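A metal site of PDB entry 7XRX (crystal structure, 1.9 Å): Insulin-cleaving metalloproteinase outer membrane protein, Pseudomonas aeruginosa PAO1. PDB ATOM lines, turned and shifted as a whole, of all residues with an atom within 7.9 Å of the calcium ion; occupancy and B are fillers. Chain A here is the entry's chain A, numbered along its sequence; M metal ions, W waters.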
ATOM      1  N   GLU A 156       4.488  21.577  10.262  1.00  0.00           N
ATOM      2  CA  GLU A 156       3.624  21.995  11.358  1.00  0.00           C
ATOM      3  C   GLU A 156       3.517  23.522  11.423  1.00  0.00           C
ATOM      4  O   GLU A 156       2.413  24.078  11.521  1.00  0.00           O
ATOM      5  CB  GLU A 156       4.143  21.422  12.677  1.00  0.00           C
ATOM      6  CG  GLU A 156       3.230  21.608  13.882  1.00  0.00           C
ATOM      7  CD  GLU A 156       3.975  21.456  15.216  1.00  0.00           C
ATOM      8  OE1 GLU A 156       5.197  21.169  15.211  1.00  0.00           O
ATOM      9  OE2 GLU A 156       3.342  21.643  16.280  1.00  0.00           O
ATOM     10  N   GLY A 161       1.002  27.961  11.995  1.00  0.00           N
ATOM     11  CA  GLY A 161       1.533  29.249  12.412  1.00  0.00           C
ATOM     12  C   GLY A 161       1.900  29.213  13.893  1.00  0.00           C
ATOM     13  O   GLY A 161       1.769  28.203  14.579  1.00  0.00           O
ATOM     14  N   GLN A 162       2.381  30.362  14.369  1.00  0.00           N
ATOM     15  CA  GLN A 162       2.760  30.468  15.774  1.00  0.00           C
ATOM     16  C   GLN A 162       1.544  30.275  16.669  1.00  0.00           C
ATOM     17  O   GLN A 162       0.447  30.727  16.366  1.00  0.00           O
ATOM     18  CB  GLN A 162       3.366  31.845  16.056  1.00  0.00           C
ATOM     19  CG  GLN A 162       4.753  32.078  15.469  1.00  0.00           C
ATOM     20  CD  GLN A 162       5.364  33.376  15.964  1.00  0.00           C
ATOM     21  OE1 GLN A 162       4.789  34.446  15.774  1.00  0.00           O
ATOM     22  NE2 GLN A 162       6.523  33.286  16.613  1.00  0.00           N
ATOM     23  N   ASP A 163       1.758  29.591  17.791  1.00  0.00           N
ATOM     24  CA  ASP A 163       0.762  29.534  18.846  1.00  0.00           C
ATOM     25  C   ASP A 163       0.900  30.796  19.695  1.00  0.00           C
ATOM     26  O   ASP A 163       1.841  30.914  20.483  1.00  0.00           O
ATOM     27  CB  ASP A 163       0.950  28.273  19.694  1.00  0.00           C
ATOM     28  CG  ASP A 163      -0.135  28.100  20.754  1.00  0.00           C
ATOM     29  OD1 ASP A 163      -0.998  28.992  20.890  1.00  0.00           O
ATOM     30  OD2 ASP A 163      -0.110  27.082  21.461  1.00  0.00           O
ATOM     31  N   LEU A 164      -0.032  31.728  19.534  1.00  0.00           N
ATOM     32  CA  LEU A 164       0.038  33.008  20.242  1.00  0.00           C
ATOM     33  C   LEU A 164      -0.640  32.962  21.608  1.00  0.00           C
ATOM     34  O   LEU A 164      -0.724  33.995  22.273  1.00  0.00           O
ATOM     35  CB  LEU A 164      -0.566  34.113  19.376  1.00  0.00           C
ATOM     36  CG  LEU A 164      -0.036  34.245  17.936  1.00  0.00           C
ATOM     37  CD1 LEU A 164      -0.895  35.199  17.115  1.00  0.00           C
ATOM     38  CD2 LEU A 164       1.419  34.690  17.921  1.00  0.00           C
ATOM     39  N   ASN A 165      -1.092  31.799  22.056  1.00  0.00           N
ATOM     40  CA  ASN A 165      -1.924  31.698  23.256  1.00  0.00           C
ATOM     41  C   ASN A 165      -1.141  31.410  24.536  1.00  0.00           C
ATOM     42  O   ASN A 165      -1.763  31.327  25.606  1.00  0.00           O
ATOM     43  CB  ASN A 165      -2.995  30.619  23.057  1.00  0.00           C
ATOM     44  CG  ASN A 165      -3.962  30.958  21.945  1.00  0.00           C
ATOM     45  OD1 ASN A 165      -4.726  31.908  22.055  1.00  0.00           O
ATOM     46  ND2 ASN A 165      -3.924  30.191  20.861  1.00  0.00           N
ATOM     47  N   GLY A 166       0.172  31.253  24.467  1.00  0.00           N
ATOM     48  CA  GLY A 166       0.961  31.079  25.688  1.00  0.00           C
ATOM     49  C   GLY A 166       0.604  29.796  26.430  1.00  0.00           C
ATOM     50  O   GLY A 166       0.642  28.707  25.853  1.00  0.00           O
ATOM     51  N   THR A 167       0.290  29.930  27.720  1.00  0.00           N
ATOM     52  CA  THR A 167      -0.194  28.816  28.532  1.00  0.00           C
ATOM     53  C   THR A 167      -1.714  28.721  28.554  1.00  0.00           C
ATOM     54  O   THR A 167      -2.270  27.964  29.353  1.00  0.00           O
ATOM     55  CB  THR A 167       0.317  28.930  29.981  1.00  0.00           C
ATOM     56  OG1 THR A 167      -0.148  30.152  30.557  1.00  0.00           O
ATOM     57  CG2 THR A 167       1.838  28.868  30.045  1.00  0.00           C
ATOM     58  N   GLY A 168      -2.401  29.490  27.707  1.00  0.00           N
ATOM     59  CA  GLY A 168      -3.836  29.427  27.634  1.00  0.00           C
ATOM     60  C   GLY A 168      -4.326  28.452  26.583  1.00  0.00           C
ATOM     61  O   GLY A 168      -3.533  27.809  25.864  1.00  0.00           O
ATOM     62  N   GLY A 170      -5.735  26.959  23.127  1.00  0.00           N
ATOM     63  CA  GLY A 170      -5.635  27.233  21.710  1.00  0.00           C
ATOM     64  C   GLY A 170      -4.226  27.018  21.158  1.00  0.00           C
ATOM     65  O   GLY A 170      -3.218  27.233  21.851  1.00  0.00           O
ATOM     66  N   ALA A 171      -4.173  26.620  19.883  1.00  0.00           N
ATOM     67  CA  ALA A 171      -2.936  26.416  19.135  1.00  0.00           C
ATOM     68  C   ALA A 171      -2.770  27.533  18.104  1.00  0.00           C
ATOM     69  O   ALA A 171      -3.456  28.558  18.152  1.00  0.00           O
ATOM     70  CB  ALA A 171      -2.940  25.033  18.477  1.00  0.00           C
ATOM     71  N   GLY A 172      -1.834  27.351  17.183  1.00  0.00           N
ATOM     72  CA  GLY A 172      -1.724  28.288  16.077  1.00  0.00           C
ATOM     73  C   GLY A 172      -2.991  28.292  15.246  1.00  0.00           C
ATOM     74  O   GLY A 172      -3.717  27.302  15.178  1.00  0.00           O
ATOM     75  N   THR A 265       6.669  27.304  27.093  1.00  0.00           N
ATOM     76  CA  THR A 265       5.863  26.749  26.017  1.00  0.00           C
ATOM     77  C   THR A 265       6.629  26.727  24.702  1.00  0.00           C
ATOM     78  O   THR A 265       6.360  25.882  23.847  1.00  0.00           O
ATOM     79  CB  THR A 265       4.573  27.550  25.847  1.00  0.00           C
ATOM     80  OG1 THR A 265       4.896  28.903  25.522  1.00  0.00           O
ATOM     81  CG2 THR A 265       3.746  27.526  27.145  1.00  0.00           C
ATOM     82  N   GLU A 266       7.575  27.637  24.528  1.00  0.00           N
ATOM     83  CA  GLU A 266       8.404  27.668  23.328  1.00  0.00           C
ATOM     84  C   GLU A 266       9.252  26.417  23.166  1.00  0.00           C
ATOM     85  O   GLU A 266       9.764  26.165  22.067  1.00  0.00           O
ATOM     86  CB  GLU A 266       9.306  28.891  23.355  1.00  0.00           C
ATOM     87  CG  GLU A 266      10.638  28.566  24.015  1.00  0.00           C
ATOM     88  CD  GLU A 266      11.542  29.745  24.176  1.00  0.00           C
ATOM     89  OE1 GLU A 266      11.643  30.228  25.333  1.00  0.00           O
ATOM     90  OE2 GLU A 266      12.191  30.158  23.172  1.00  0.00           O
ATOM     91  N   GLU A 268       8.116  23.218  23.934  1.00  0.00           N
ATOM     92  CA  GLU A 268       7.366  21.967  23.801  1.00  0.00           C
ATOM     93  C   GLU A 268       7.561  21.401  22.406  1.00  0.00           C
ATOM     94  O   GLU A 268       7.850  22.122  21.451  1.00  0.00           O
ATOM     95  CB  GLU A 268       5.880  22.188  24.096  1.00  0.00           C
ATOM     96  CG  GLU A 268       5.164  23.037  23.059  1.00  0.00           C
ATOM     97  CD  GLU A 268       3.648  22.906  23.132  1.00  0.00           C
ATOM     98  OE1 GLU A 268       3.145  21.817  23.479  1.00  0.00           O
ATOM     99  OE2 GLU A 268       2.967  23.912  22.857  1.00  0.00           O
ATOM    100  N   ASP A 270       5.655  19.904  20.039  1.00  0.00           N
ATOM    101  CA  ASP A 270       4.745  20.288  18.961  1.00  0.00           C
ATOM    102  C   ASP A 270       4.135  21.640  19.312  1.00  0.00           C
ATOM    103  O   ASP A 270       2.966  21.752  19.683  1.00  0.00           O
ATOM    104  CB  ASP A 270       3.688  19.195  18.742  1.00  0.00           C
ATOM    105  CG  ASP A 270       4.302  17.821  18.531  1.00  0.00           C
ATOM    106  OD1 ASP A 270       4.725  17.503  17.400  1.00  0.00           O
ATOM    107  OD2 ASP A 270       4.392  17.053  19.521  1.00  0.00           O
ATOM    108  N   CYS A 271       4.973  22.669  19.178  1.00  0.00           N
ATOM    109  CA  CYS A 271       4.674  24.019  19.633  1.00  0.00           C
ATOM    110  C   CYS A 271       3.396  24.567  19.005  1.00  0.00           C
ATOM    111  O   CYS A 271       2.562  25.192  19.700  1.00  0.00           O
ATOM    112  CB  CYS A 271       5.860  24.925  19.295  1.00  0.00           C
ATOM    113  SG  CYS A 271       5.784  26.617  19.861  1.00  0.00           S
ATOM    114  N   PHE A 272       3.228  24.365  17.705  1.00  0.00           N
ATOM    115  CA  PHE A 272       2.220  25.099  16.945  1.00  0.00           C
ATOM    116  C   PHE A 272       0.877  24.373  16.892  1.00  0.00           C
ATOM    117  O   PHE A 272      -0.175  25.012  16.944  1.00  0.00           O
ATOM    118  CB  PHE A 272       2.755  25.344  15.536  1.00  0.00           C
ATOM    119  CG  PHE A 272       4.214  25.740  15.511  1.00  0.00           C
ATOM    120  CD1 PHE A 272       4.595  26.999  15.957  1.00  0.00           C
ATOM    121  CD2 PHE A 272       5.186  24.859  15.070  1.00  0.00           C
ATOM    122  CE1 PHE A 272       5.943  27.379  15.948  1.00  0.00           C
ATOM    123  CE2 PHE A 272       6.523  25.225  15.064  1.00  0.00           C
ATOM    124  CZ  PHE A 272       6.902  26.492  15.503  1.00  0.00           C
ATOM    125  N   SER A 273       0.904  23.048  16.814  1.00  0.00           N
ATOM    126  CA  SER A 273      -0.297  22.230  16.756  1.00  0.00           C
ATOM    127  C   SER A 273      -0.776  21.806  18.135  1.00  0.00           C
ATOM    128  O   SER A 273      -1.913  21.330  18.249  1.00  0.00           O
ATOM    129  CB  SER A 273      -0.049  20.985  15.918  1.00  0.00           C
ATOM    130  OG  SER A 273       0.913  20.168  16.557  1.00  0.00           O
ATOM    131  N   ASP A 274       0.066  21.934  19.158  1.00  0.00           N
ATOM    132  CA  ASP A 274      -0.242  21.494  20.516  1.00  0.00           C
ATOM    133  C   ASP A 274      -0.520  19.993  20.590  1.00  0.00           C
ATOM    134  O   ASP A 274      -1.300  19.537  21.435  1.00  0.00           O
ATOM    135  CB  ASP A 274      -1.386  22.305  21.111  1.00  0.00           C
ATOM    136  CG  ASP A 274      -0.984  23.727  21.411  1.00  0.00           C
ATOM    137  OD1 ASP A 274       0.239  23.985  21.426  1.00  0.00           O
ATOM    138  OD2 ASP A 274      -1.869  24.590  21.643  1.00  0.00           O
ATOM    139  N   ASP A 275       0.151  19.207  19.753  1.00  0.00           N
ATOM    140  CA  ASP A 275       0.037  17.755  19.743  1.00  0.00           C
ATOM    141  C   ASP A 275       1.072  17.082  20.637  1.00  0.00           C
ATOM    142  O   ASP A 275       1.241  15.849  20.558  1.00  0.00           O
ATOM    143  CB  ASP A 275       0.167  17.241  18.304  1.00  0.00           C
ATOM    144  CG  ASP A 275      -0.461  15.872  18.112  1.00  0.00           C
ATOM    145  OD1 ASP A 275      -1.498  15.614  18.735  1.00  0.00           O
ATOM    146  OD2 ASP A 275       0.098  15.070  17.320  1.00  0.00           O
ATOM    147  N   THR A 276       1.752  17.849  21.499  1.00  0.00           N
ATOM    148  CA  THR A 276       2.878  17.307  22.269  1.00  0.00           C
ATOM    149  C   THR A 276       2.489  16.068  23.067  1.00  0.00           C
ATOM    150  O   THR A 276       3.294  15.142  23.197  1.00  0.00           O
ATOM    151  CB  THR A 276       3.443  18.385  23.185  1.00  0.00           C
ATOM    152  OG1 THR A 276       3.894  19.501  22.400  1.00  0.00           O
ATOM    153  CG2 THR A 276       4.623  17.847  23.988  1.00  0.00           C
ATOM    154  N   HIS A 347      -4.005  21.127  27.108  1.00  0.00           N
ATOM    155  CA  HIS A 347      -2.875  20.609  26.368  1.00  0.00           C
ATOM    156  C   HIS A 347      -1.573  20.815  27.147  1.00  0.00           C
ATOM    157  O   HIS A 347      -1.555  21.416  28.231  1.00  0.00           O
ATOM    158  CB  HIS A 347      -2.824  21.238  24.975  1.00  0.00           C
ATOM    159  CG  HIS A 347      -3.891  20.745  24.057  1.00  0.00           C
ATOM    160  ND1 HIS A 347      -3.620  20.180  22.823  1.00  0.00           N
ATOM    161  CD2 HIS A 347      -5.244  20.712  24.188  1.00  0.00           C
ATOM    162  CE1 HIS A 347      -4.745  19.829  22.242  1.00  0.00           C
ATOM    163  NE2 HIS A 347      -5.748  20.143  23.039  1.00  0.00           N
ATOM    164  N   PHE A 348      -0.472  20.290  26.603  1.00  0.00           N
ATOM    165  CA  PHE A 348       0.798  20.315  27.314  1.00  0.00           C
ATOM    166  C   PHE A 348       1.223  21.736  27.651  1.00  0.00           C
ATOM    167  O   PHE A 348       1.727  21.994  28.748  1.00  0.00           O
ATOM    168  CB  PHE A 348       1.876  19.601  26.482  1.00  0.00           C
ATOM    169  CG  PHE A 348       3.208  19.439  27.182  1.00  0.00           C
ATOM    170  CD1 PHE A 348       3.396  18.439  28.119  1.00  0.00           C
ATOM    171  CD2 PHE A 348       4.282  20.266  26.866  1.00  0.00           C
ATOM    172  CE1 PHE A 348       4.629  18.268  28.748  1.00  0.00           C
ATOM    173  CE2 PHE A 348       5.504  20.116  27.493  1.00  0.00           C
ATOM    174  CZ  PHE A 348       5.685  19.110  28.438  1.00  0.00           C
ATOM    175  N   ASP A 349       1.026  22.686  26.724  1.00  0.00           N
ATOM    176  CA  ASP A 349       1.435  24.052  27.021  1.00  0.00           C
ATOM    177  C   ASP A 349       0.601  24.673  28.148  1.00  0.00           C
ATOM    178  O   ASP A 349       1.038  25.660  28.733  1.00  0.00           O
ATOM    179  CB  ASP A 349       1.414  24.932  25.756  1.00  0.00           C
ATOM    180  CG  ASP A 349       0.081  24.918  25.014  1.00  0.00           C
ATOM    181  OD1 ASP A 349      -0.907  24.389  25.540  1.00  0.00           O
ATOM    182  OD2 ASP A 349       0.038  25.458  23.883  1.00  0.00           O
ATOM    183  N   GLN A 350      -0.550  24.090  28.482  1.00  0.00           N
ATOM    184  CA  GLN A 350      -1.346  24.526  29.622  1.00  0.00           C
ATOM    185  C   GLN A 350      -0.949  23.825  30.913  1.00  0.00           C
ATOM    186  O   GLN A 350      -0.975  24.435  31.990  1.00  0.00           O
ATOM    187  CB  GLN A 350      -2.827  24.303  29.344  1.00  0.00           C
ATOM    188  CG  GLN A 350      -3.346  25.073  28.150  1.00  0.00           C
ATOM    189  CD  GLN A 350      -4.672  24.554  27.655  1.00  0.00           C
ATOM    190  OE1 GLN A 350      -4.719  23.770  26.696  1.00  0.00           O
ATOM    191  NE2 GLN A 350      -5.755  24.979  28.295  1.00  0.00           N
HETATM  192 CA    CA M   1       1.759  25.634  21.994  1.00  0.00          CA
HETATM  193  O   HOH W   1       3.756  27.081  21.602  1.00  0.00           O
HETATM  194  O   HOH W   2       2.251  27.651  23.652  1.00  0.00           O
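OG1 of Thr 276 sits at hydrogen-bond distance from OE1 of Glu 268 (2.7 Å). The backbone NH (N) of Cys 271 sits at hydrogen-bond distance from the side-chain carboxylate (OE2) of Glu 156, at 3.5 Å. The side-chain carboxylate (OD1) of Asp 163 sits at hydrogen-bond distance from the backbone NH (N) of Asn 165 (3.0 Å). The backbone carbonyl oxygen (O) of Asp 274 is in hydrogen-bond range of a ring nitrogen (ND1) of His 347 (2.8 Å).
Five residues have an atom within 4 Å of the calcium ion: Asp 163, Glu 268, Cys 271, Asp 274 and Asp 349. The nearest printed residue that does not touch the calcium ion is Asp 270 (4.7 Å).
OE2 of Glu 268 binds the calcium ion (2.3 Å). The calcium ion is bound by OD1 of Asp 274, at 2.3 Å. OD2 of Asp 163 is bound to the calcium ion (2.4 Å). O of Cys 271 binds the calcium ion, 2.5 Å away. The calcium ion is bound by water W1, at 2.5 Å. OD2 of Asp 349 binds the calcium ion, at 2.6 Å. The calcium ion is bound by water W2 (2.7 Å). The calcium ion has seven donor atoms within binding distance.
Water W2 lies within hydrogen-bond range of the backbone carbonyl oxygen of Gly 166 (2.9 Å) and the side-chain hydroxyl of Thr 265 (3.5 Å).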
